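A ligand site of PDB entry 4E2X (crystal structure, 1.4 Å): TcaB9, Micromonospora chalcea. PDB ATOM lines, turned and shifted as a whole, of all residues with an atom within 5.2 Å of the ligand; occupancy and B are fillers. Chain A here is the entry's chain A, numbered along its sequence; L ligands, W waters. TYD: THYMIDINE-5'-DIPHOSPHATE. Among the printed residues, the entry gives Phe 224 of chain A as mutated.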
ATOM      1  N   ASP A  35     -31.598  -6.308 -14.963  1.00  0.00           N
ATOM      2  CA  ASP A  35     -31.326  -5.046 -15.637  1.00  0.00           C
ATOM      3  C   ASP A  35     -31.662  -3.865 -14.747  1.00  0.00           C
ATOM      4  O   ASP A  35     -31.737  -2.706 -15.203  1.00  0.00           O
ATOM      5  CB  ASP A  35     -31.997  -4.916 -17.010  1.00  0.00           C
ATOM      6  CG  ASP A  35     -31.121  -5.426 -18.139  1.00  0.00           C
ATOM      7  OD1 ASP A  35     -29.987  -4.943 -18.142  1.00  0.00           O
ATOM      8  OD2 ASP A  35     -31.571  -6.223 -18.968  1.00  0.00           O
ATOM      9  N   TYR A  80     -30.979  -1.460 -21.581  1.00  0.00           N
ATOM     10  CA  TYR A  80     -30.095  -2.109 -22.578  1.00  0.00           C
ATOM     11  C   TYR A  80     -30.206  -1.311 -23.870  1.00  0.00           C
ATOM     12  O   TYR A  80     -31.328  -1.131 -24.392  1.00  0.00           O
ATOM     13  CB  TYR A  80     -30.658  -3.480 -22.963  1.00  0.00           C
ATOM     14  CG  TYR A  80     -29.719  -4.227 -23.894  1.00  0.00           C
ATOM     15  CD1 TYR A  80     -28.419  -4.543 -23.498  1.00  0.00           C
ATOM     16  CD2 TYR A  80     -30.107  -4.589 -25.200  1.00  0.00           C
ATOM     17  CE1 TYR A  80     -27.514  -5.245 -24.326  1.00  0.00           C
ATOM     18  CE2 TYR A  80     -29.227  -5.278 -26.019  1.00  0.00           C
ATOM     19  CZ  TYR A  80     -27.974  -5.549 -25.590  1.00  0.00           C
ATOM     20  OH  TYR A  80     -27.225  -6.267 -26.463  1.00  0.00           O
ATOM     21  N   GLY A  84     -25.247  -0.242 -28.827  1.00  0.00           N
ATOM     22  CA  GLY A  84     -23.902  -0.187 -28.272  1.00  0.00           C
ATOM     23  C   GLY A  84     -22.881  -1.175 -28.816  1.00  0.00           C
ATOM     24  O   GLY A  84     -21.722  -1.117 -28.414  1.00  0.00           O
ATOM     25  N   SER A  85     -23.212  -2.047 -29.764  1.00  0.00           N
ATOM     26  CA  SER A  85     -22.179  -2.960 -30.226  1.00  0.00           C
ATOM     27  C   SER A  85     -22.139  -2.742 -31.746  1.00  0.00           C
ATOM     28  O   SER A  85     -23.183  -2.832 -32.406  1.00  0.00           O
ATOM     29  CB  SER A  85     -22.730  -4.377 -30.019  1.00  0.00           C
ATOM     30  OG  SER A  85     -22.044  -5.321 -30.859  1.00  0.00           O
ATOM     31  N   PHE A 224     -31.502 -16.031 -16.893  1.00  0.00           N
ATOM     32  CA  PHE A 224     -31.868 -14.900 -16.011  1.00  0.00           C
ATOM     33  C   PHE A 224     -33.279 -14.448 -16.324  1.00  0.00           C
ATOM     34  O   PHE A 224     -33.912 -15.034 -17.215  1.00  0.00           O
ATOM     35  CB  PHE A 224     -30.837 -13.766 -16.118  1.00  0.00           C
ATOM     36  CG  PHE A 224     -30.639 -13.180 -17.494  1.00  0.00           C
ATOM     37  CD1 PHE A 224     -31.267 -12.007 -17.882  1.00  0.00           C
ATOM     38  CD2 PHE A 224     -29.793 -13.783 -18.402  1.00  0.00           C
ATOM     39  CE1 PHE A 224     -31.066 -11.431 -19.133  1.00  0.00           C
ATOM     40  CE2 PHE A 224     -29.568 -13.201 -19.631  1.00  0.00           C
ATOM     41  CZ  PHE A 224     -30.247 -12.068 -20.032  1.00  0.00           C
ATOM     42  N   HIS A 256     -24.387 -13.162 -29.573  1.00  0.00           N
ATOM     43  CA  HIS A 256     -24.867 -13.445 -28.243  1.00  0.00           C
ATOM     44  C   HIS A 256     -24.647 -14.831 -27.675  1.00  0.00           C
ATOM     45  O   HIS A 256     -25.456 -15.394 -26.927  1.00  0.00           O
ATOM     46  CB  HIS A 256     -26.343 -13.092 -28.128  1.00  0.00           C
ATOM     47  CG  HIS A 256     -26.583 -11.618 -28.229  1.00  0.00           C
ATOM     48  ND1 HIS A 256     -26.099 -10.714 -27.302  1.00  0.00           N
ATOM     49  CD2 HIS A 256     -27.268 -10.883 -29.134  1.00  0.00           C
ATOM     50  CE1 HIS A 256     -26.440  -9.491 -27.665  1.00  0.00           C
ATOM     51  NE2 HIS A 256     -27.179  -9.570 -28.748  1.00  0.00           N
ATOM     52  N   TYR A 325     -15.565  -6.615 -16.922  1.00  0.00           N
ATOM     53  CA  TYR A 325     -15.726  -5.857 -18.161  1.00  0.00           C
ATOM     54  C   TYR A 325     -17.067  -6.232 -18.785  1.00  0.00           C
ATOM     55  O   TYR A 325     -17.309  -7.373 -19.156  1.00  0.00           O
ATOM     56  CB  TYR A 325     -14.545  -6.131 -19.099  1.00  0.00           C
ATOM     57  CG  TYR A 325     -14.406  -4.994 -20.114  1.00  0.00           C
ATOM     58  CD1 TYR A 325     -15.454  -4.714 -21.008  1.00  0.00           C
ATOM     59  CD2 TYR A 325     -13.259  -4.194 -20.128  1.00  0.00           C
ATOM     60  CE1 TYR A 325     -15.358  -3.656 -21.923  1.00  0.00           C
ATOM     61  CE2 TYR A 325     -13.149  -3.134 -21.040  1.00  0.00           C
ATOM     62  CZ  TYR A 325     -14.184  -2.893 -21.940  1.00  0.00           C
ATOM     63  OH  TYR A 325     -14.058  -1.849 -22.851  1.00  0.00           O
ATOM     64  N   GLY A 326     -17.965  -5.261 -18.792  1.00  0.00           N
ATOM     65  CA  GLY A 326     -19.315  -5.355 -19.370  1.00  0.00           C
ATOM     66  C   GLY A 326     -20.286  -5.519 -18.219  1.00  0.00           C
ATOM     67  O   GLY A 326     -20.266  -6.536 -17.535  1.00  0.00           O
ATOM     68  N   ALA A 327     -21.155  -4.528 -17.950  1.00  0.00           N
ATOM     69  CA  ALA A 327     -22.228  -4.667 -16.950  1.00  0.00           C
ATOM     70  C   ALA A 327     -23.427  -5.382 -17.564  1.00  0.00           C
ATOM     71  O   ALA A 327     -24.507  -4.829 -17.709  1.00  0.00           O
ATOM     72  CB  ALA A 327     -22.662  -3.334 -16.326  1.00  0.00           C
ATOM     73  N   THR A 328     -23.244  -6.653 -17.921  1.00  0.00           N
ATOM     74  CA  THR A 328     -24.222  -7.420 -18.703  1.00  0.00           C
ATOM     75  C   THR A 328     -25.379  -7.739 -17.765  1.00  0.00           C
ATOM     76  O   THR A 328     -25.145  -7.918 -16.567  1.00  0.00           O
ATOM     77  CB  THR A 328     -23.541  -8.711 -19.206  1.00  0.00           C
ATOM     78  OG1 THR A 328     -23.076  -9.390 -18.037  1.00  0.00           O
ATOM     79  CG2 THR A 328     -22.400  -8.494 -20.263  1.00  0.00           C
ATOM     80  N   ALA A 329     -26.604  -7.841 -18.281  1.00  0.00           N
ATOM     81  CA  ALA A 329     -27.737  -8.486 -17.644  1.00  0.00           C
ATOM     82  C   ALA A 329     -27.355  -9.901 -17.178  1.00  0.00           C
ATOM     83  O   ALA A 329     -27.612 -10.354 -16.066  1.00  0.00           O
ATOM     84  CB  ALA A 329     -28.900  -8.537 -18.590  1.00  0.00           C
ATOM     85  N   LYS A 330     -26.626 -10.565 -18.086  1.00  0.00           N
ATOM     86  CA  LYS A 330     -26.108 -11.931 -17.910  1.00  0.00           C
ATOM     87  C   LYS A 330     -25.311 -12.092 -16.604  1.00  0.00           C
ATOM     88  O   LYS A 330     -25.407 -13.103 -15.888  1.00  0.00           O
ATOM     89  CB  LYS A 330     -25.208 -12.431 -19.054  1.00  0.00           C
ATOM     90  CG  LYS A 330     -25.994 -12.665 -20.362  1.00  0.00           C
ATOM     91  CD  LYS A 330     -25.140 -13.401 -21.413  1.00  0.00           C
ATOM     92  CE  LYS A 330     -23.924 -12.599 -21.861  1.00  0.00           C
ATOM     93  NZ  LYS A 330     -24.246 -11.344 -22.610  1.00  0.00           N
ATOM     94  N   TYR A 349     -16.577  -2.204 -15.847  1.00  0.00           N
ATOM     95  CA  TYR A 349     -16.504  -1.147 -16.859  1.00  0.00           C
ATOM     96  C   TYR A 349     -17.545  -1.385 -17.945  1.00  0.00           C
ATOM     97  O   TYR A 349     -17.771  -2.511 -18.394  1.00  0.00           O
ATOM     98  CB  TYR A 349     -15.069  -1.123 -17.382  1.00  0.00           C
ATOM     99  CG  TYR A 349     -14.182  -0.704 -16.235  1.00  0.00           C
ATOM    100  CD1 TYR A 349     -14.117   0.629 -15.848  1.00  0.00           C
ATOM    101  CD2 TYR A 349     -13.489  -1.661 -15.500  1.00  0.00           C
ATOM    102  CE1 TYR A 349     -13.334   0.989 -14.765  1.00  0.00           C
ATOM    103  CE2 TYR A 349     -12.704  -1.319 -14.419  1.00  0.00           C
ATOM    104  CZ  TYR A 349     -12.606   0.023 -14.088  1.00  0.00           C
ATOM    105  OH  TYR A 349     -11.858   0.361 -13.002  1.00  0.00           O
ATOM    106  N   ASP A 350     -18.259  -0.308 -18.293  1.00  0.00           N
ATOM    107  CA  ASP A 350     -19.329  -0.472 -19.275  1.00  0.00           C
ATOM    108  C   ASP A 350     -19.583   0.820 -20.090  1.00  0.00           C
ATOM    109  O   ASP A 350     -19.459   1.917 -19.518  1.00  0.00           O
ATOM    110  CB  ASP A 350     -20.630  -0.740 -18.511  1.00  0.00           C
ATOM    111  CG  ASP A 350     -21.704  -1.284 -19.429  1.00  0.00           C
ATOM    112  OD1 ASP A 350     -21.755  -2.529 -19.681  1.00  0.00           O
ATOM    113  OD2 ASP A 350     -22.480  -0.420 -19.893  1.00  0.00           O
ATOM    114  N   THR A 351     -19.961   0.720 -21.365  1.00  0.00           N
ATOM    115  CA  THR A 351     -20.148   1.906 -22.200  1.00  0.00           C
ATOM    116  C   THR A 351     -21.544   2.503 -22.100  1.00  0.00           C
ATOM    117  O   THR A 351     -21.819   3.479 -22.796  1.00  0.00           O
ATOM    118  CB  THR A 351     -19.939   1.554 -23.656  1.00  0.00           C
ATOM    119  OG1 THR A 351     -20.646   0.348 -23.991  1.00  0.00           O
ATOM    120  CG2 THR A 351     -18.477   1.308 -23.866  1.00  0.00           C
ATOM    121  N   THR A 352     -22.436   1.932 -21.303  1.00  0.00           N
ATOM    122  CA  THR A 352     -23.828   2.371 -21.250  1.00  0.00           C
ATOM    123  C   THR A 352     -24.015   3.473 -20.198  1.00  0.00           C
ATOM    124  O   THR A 352     -23.919   3.213 -18.994  1.00  0.00           O
ATOM    125  CB  THR A 352     -24.835   1.200 -20.958  1.00  0.00           C
ATOM    126  OG1 THR A 352     -24.482   0.006 -21.682  1.00  0.00           O
ATOM    127  CG2 THR A 352     -26.302   1.545 -21.265  1.00  0.00           C
ATOM    128  N   LYS A 355     -26.045   2.817 -17.029  1.00  0.00           N
ATOM    129  CA  LYS A 355     -25.561   1.836 -16.045  1.00  0.00           C
ATOM    130  C   LYS A 355     -24.335   2.409 -15.312  1.00  0.00           C
ATOM    131  O   LYS A 355     -23.959   1.870 -14.270  1.00  0.00           O
ATOM    132  CB  LYS A 355     -25.074   0.559 -16.774  1.00  0.00           C
ATOM    133  CG  LYS A 355     -26.190  -0.191 -17.531  1.00  0.00           C
ATOM    134  CD  LYS A 355     -25.586  -1.474 -18.158  1.00  0.00           C
ATOM    135  CE  LYS A 355     -26.674  -2.225 -18.939  1.00  0.00           C
ATOM    136  NZ  LYS A 355     -26.165  -3.505 -19.533  1.00  0.00           N
ATOM    137  N   ALA A 370     -16.309   2.794 -19.498  1.00  0.00           N
ATOM    138  CA  ALA A 370     -15.248   1.962 -20.033  1.00  0.00           C
ATOM    139  C   ALA A 370     -14.049   2.853 -20.269  1.00  0.00           C
ATOM    140  O   ALA A 370     -12.912   2.363 -20.290  1.00  0.00           O
ATOM    141  CB  ALA A 370     -15.705   1.364 -21.342  1.00  0.00           C
ATOM    142  N   ALA A 385     -18.906  -9.573 -20.680  1.00  0.00           N
ATOM    143  CA  ALA A 385     -19.382  -9.437 -22.051  1.00  0.00           C
ATOM    144  C   ALA A 385     -18.593 -10.379 -22.971  1.00  0.00           C
ATOM    145  O   ALA A 385     -18.050  -9.922 -23.993  1.00  0.00           O
ATOM    146  CB  ALA A 385     -19.328  -7.973 -22.476  1.00  0.00           C
ATOM    147  N   ASN A 387     -19.535 -12.637 -25.034  1.00  0.00           N
ATOM    148  CA  ASN A 387     -20.101 -12.724 -26.386  1.00  0.00           C
ATOM    149  C   ASN A 387     -19.612 -11.600 -27.305  1.00  0.00           C
ATOM    150  O   ASN A 387     -19.865 -11.684 -28.524  1.00  0.00           O
ATOM    151  CB  ASN A 387     -21.641 -12.722 -26.283  1.00  0.00           C
ATOM    152  CG  ASN A 387     -22.184 -11.606 -25.408  1.00  0.00           C
ATOM    153  OD1 ASN A 387     -21.881 -11.485 -24.204  1.00  0.00           O
ATOM    154  ND2 ASN A 387     -23.023 -10.793 -26.033  1.00  0.00           N
ATOM    155  N   HIS A 388     -18.978 -10.569 -26.744  1.00  0.00           N
ATOM    156  CA  HIS A 388     -18.438  -9.416 -27.469  1.00  0.00           C
ATOM    157  C   HIS A 388     -16.926  -9.398 -27.384  1.00  0.00           C
ATOM    158  O   HIS A 388     -16.278  -8.351 -27.560  1.00  0.00           O
ATOM    159  CB  HIS A 388     -18.922  -8.116 -26.868  1.00  0.00           C
ATOM    160  CG  HIS A 388     -20.408  -7.889 -26.987  1.00  0.00           C
ATOM    161  ND1 HIS A 388     -21.022  -7.714 -28.206  1.00  0.00           N
ATOM    162  CD2 HIS A 388     -21.385  -7.830 -26.055  1.00  0.00           C
ATOM    163  CE1 HIS A 388     -22.314  -7.501 -28.033  1.00  0.00           C
ATOM    164  NE2 HIS A 388     -22.554  -7.583 -26.737  1.00  0.00           N
ATOM    165  N   GLU A 391     -14.921  -7.752 -30.293  1.00  0.00           N
ATOM    166  CA  GLU A 391     -15.099  -6.316 -30.462  1.00  0.00           C
ATOM    167  C   GLU A 391     -14.446  -5.572 -29.294  1.00  0.00           C
ATOM    168  O   GLU A 391     -13.820  -4.515 -29.477  1.00  0.00           O
ATOM    169  CB  GLU A 391     -16.601  -6.040 -30.499  1.00  0.00           C
ATOM    170  CG  GLU A 391     -16.966  -4.568 -30.482  1.00  0.00           C
ATOM    171  CD  GLU A 391     -18.443  -4.295 -30.708  1.00  0.00           C
ATOM    172  OE1 GLU A 391     -18.837  -3.135 -30.502  1.00  0.00           O
ATOM    173  OE2 GLU A 391     -19.225  -5.204 -31.070  1.00  0.00           O
ATOM    174  N   ILE A 392     -14.565  -6.138 -28.092  1.00  0.00           N
ATOM    175  CA  ILE A 392     -14.040  -5.470 -26.900  1.00  0.00           C
ATOM    176  C   ILE A 392     -12.515  -5.537 -26.942  1.00  0.00           C
ATOM    177  O   ILE A 392     -11.857  -4.506 -26.741  1.00  0.00           O
ATOM    178  CB  ILE A 392     -14.600  -6.059 -25.595  1.00  0.00           C
ATOM    179  CG1 ILE A 392     -16.005  -5.493 -25.404  1.00  0.00           C
ATOM    180  CG2 ILE A 392     -13.743  -5.528 -24.432  1.00  0.00           C
ATOM    181  CD1 ILE A 392     -16.778  -6.271 -24.305  1.00  0.00           C
ATOM    182  N   LYS A 395     -10.629  -3.122 -29.034  1.00  0.00           N
ATOM    183  CA  LYS A 395     -10.581  -1.762 -28.505  1.00  0.00           C
ATOM    184  C   LYS A 395      -9.670  -1.657 -27.284  1.00  0.00           C
ATOM    185  O   LYS A 395      -9.357  -0.557 -26.821  1.00  0.00           O
ATOM    186  CB  LYS A 395     -11.973  -1.310 -28.078  1.00  0.00           C
ATOM    187  CG  LYS A 395     -12.891  -1.122 -29.267  1.00  0.00           C
ATOM    188  CD  LYS A 395     -14.112  -0.357 -28.837  1.00  0.00           C
ATOM    189  CE  LYS A 395     -15.134  -1.294 -28.245  1.00  0.00           C
ATOM    190  NZ  LYS A 395     -16.280  -0.419 -27.843  1.00  0.00           N
HETATM  191  PA  TYD L   1     -24.682  -7.760 -23.960  1.00  0.00           P
HETATM  192  O1A TYD L   1     -24.954  -7.141 -25.296  1.00  0.00           O
HETATM  193  O2A TYD L   1     -23.675  -8.882 -23.954  1.00  0.00           O
HETATM  194  O3A TYD L   1     -26.141  -8.090 -23.377  1.00  0.00           O
HETATM  195  PB  TYD L   1     -26.598  -8.475 -21.865  1.00  0.00           P
HETATM  196  O1B TYD L   1     -26.831  -7.234 -21.045  1.00  0.00           O
HETATM  197  O2B TYD L   1     -25.705  -9.514 -21.247  1.00  0.00           O
HETATM  198  O3B TYD L   1     -27.877  -9.189 -22.273  1.00  0.00           O
HETATM  199  O5' TYD L   1     -24.156  -6.623 -22.970  1.00  0.00           O
HETATM  200  C5' TYD L   1     -22.874  -6.074 -23.191  1.00  0.00           C
HETATM  201  C4' TYD L   1     -22.708  -4.961 -22.168  1.00  0.00           C
HETATM  202  O4' TYD L   1     -21.348  -4.658 -22.331  1.00  0.00           O
HETATM  203  C3' TYD L   1     -23.529  -3.693 -22.373  1.00  0.00           C
HETATM  204  O3' TYD L   1     -23.915  -3.148 -21.102  1.00  0.00           O
HETATM  205  C2' TYD L   1     -22.529  -2.780 -23.057  1.00  0.00           C
HETATM  206  C1' TYD L   1     -21.138  -3.283 -22.656  1.00  0.00           C
HETATM  207  N1  TYD L   1     -20.142  -3.197 -23.753  1.00  0.00           N
HETATM  208  C2  TYD L   1     -19.000  -2.416 -23.556  1.00  0.00           C
HETATM  209  O2  TYD L   1     -18.838  -1.848 -22.455  1.00  0.00           O
HETATM  210  N3  TYD L   1     -18.081  -2.276 -24.519  1.00  0.00           N
HETATM  211  C4  TYD L   1     -18.245  -2.823 -25.724  1.00  0.00           C
HETATM  212  O4  TYD L   1     -17.379  -2.713 -26.625  1.00  0.00           O
HETATM  213  C5  TYD L   1     -19.434  -3.675 -25.975  1.00  0.00           C
HETATM  214  C5M TYD L   1     -19.631  -4.350 -27.309  1.00  0.00           C
HETATM  215  C6  TYD L   1     -20.364  -3.801 -24.933  1.00  0.00           C
HETATM  216  O   HOH W   1     -28.267  -5.042 -20.285  1.00  0.00           O
HETATM  217  O   HOH W   2     -23.733  -4.229 -26.285  1.00  0.00           O
HETATM  218  O   HOH W   3     -19.943  -0.048 -26.611  1.00  0.00           O
HETATM  219  O   HOH W   4     -15.802  -0.699 -24.423  1.00  0.00           O
HETATM  220  O   HOH W   5     -25.090  -2.103 -25.211  1.00  0.00           O
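The side-chain carboxylate (OD1) of Asp 350 sits at hydrogen-bond distance from an oxygen (O3') of the ligand. The side-chain hydroxyl of Tyr 80 lies within hydrogen-bond range of an oxygen (O1A) of the ligand, at 2.7 Å. The backbone NH of Lys 330 lies close to an oxygen (O2B) of the ligand, 3.5 Å away. NZ of Lys 330 lies within salt-bridge range of O2B of the ligand (2.7 Å). NZ of Lys 355 lies within hydrogen-bond range of O3' of the ligand, at 2.8 Å. NZ of Lys 395 is in hydrogen-bond range of O4 of the ligand, 2.8 Å away. An oxygen (O1A) of the ligand sits at hydrogen-bond distance from a ring nitrogen (NE2) of His 388, 2.8 Å away. N of Ala 329 lies within hydrogen-bond range of O1B of the ligand (2.8 Å). The side-chain amide nitrogen (ND2) of Asn 387 lies within hydrogen-bond range of an oxygen (O2A) of the ligand (2.9 Å). The backbone NH (N) of Thr 351 lies within hydrogen-bond range of an oxygen (O2) of the ligand (3.0 Å). The side-chain hydroxyl (OG1) of Thr 351 lies within hydrogen-bond range of an oxygen (O2) of the ligand, at 3.2 Å. OG1 of Thr 352 sits at hydrogen-bond distance from O3' of the ligand.
The side-chain carboxylate of Asp 350 lies within hydrogen-bond range of the side-chain hydroxyl of Thr 352, at 2.7 Å. The side-chain carboxylate (OD1) of Asp 350 is in hydrogen-bond range of the backbone NH (N) of Ala 327 (2.7 Å). The backbone NH (N) of Ala 370 lies within hydrogen-bond range of the backbone carbonyl oxygen (O) of Asp 350 (3.3 Å). The side-chain amino group (NZ) of Lys 330 sits at hydrogen-bond distance from the side-chain amide oxygen (OD1) of Asn 387 (2.9 Å). The side-chain amide nitrogen (ND2) of Asn 387 is in hydrogen-bond range of a ring nitrogen (NE2) of His 388 (3.3 Å). A ring nitrogen (ND1) of His 256 is in hydrogen-bond range of the side-chain amide nitrogen (ND2) of Asn 387 (3.3 Å). The backbone carbonyl oxygen of Tyr 349 sits at hydrogen-bond distance from the backbone NH of Gly 326 (2.8 Å). The backbone carbonyl oxygen (O) of Tyr 325 lies within hydrogen-bond range of the backbone NH (N) of Ala 385, at 3.1 Å.
His 256 touches the ligand (CE1 to O1A, 3.7 Å). CE1 of Tyr 325 touches O2 of the ligand (3.96 Å). Gly 326 touches the ligand. O of Ala 327 touches O3' of the ligand (3.8 Å). Thr 328 touches the ligand (CB to O2B, 3.1 Å). Ala 385 touches the ligand. OE1 of Glu 391 touches C5M of the ligand, 3.5 Å away. CG1 of Ile 392 touches O4 of the ligand, 3.3 Å away. Within 4 Å of the ligand: Tyr 80, His 256, Tyr 325, Gly 326, Ala 327, Thr 328, Ala 329, Lys 330, Asp 350, Thr 351, Thr 352, Lys 355, Ala 385, Asn 387, His 388, Glu 391, Ile 392 and Lys 395.
Water W1 lies within hydrogen-bond range of NZ of Lys 355 (2.7 Å), O1B of the ligand (2.7 Å) and OD1 of Asp 35 (2.7 Å). Water W4 lies within hydrogen-bond range of the side-chain hydroxyl (OH) of Tyr 325 (2.6 Å), a nitrogen (N3) of the ligand (2.8 Å) and the side-chain amino group (NZ) of Lys 395 (3.5 Å). Water W3 lies within hydrogen-bond range of the side-chain hydroxyl of Thr 351 and the backbone carbonyl oxygen of Gly 84.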
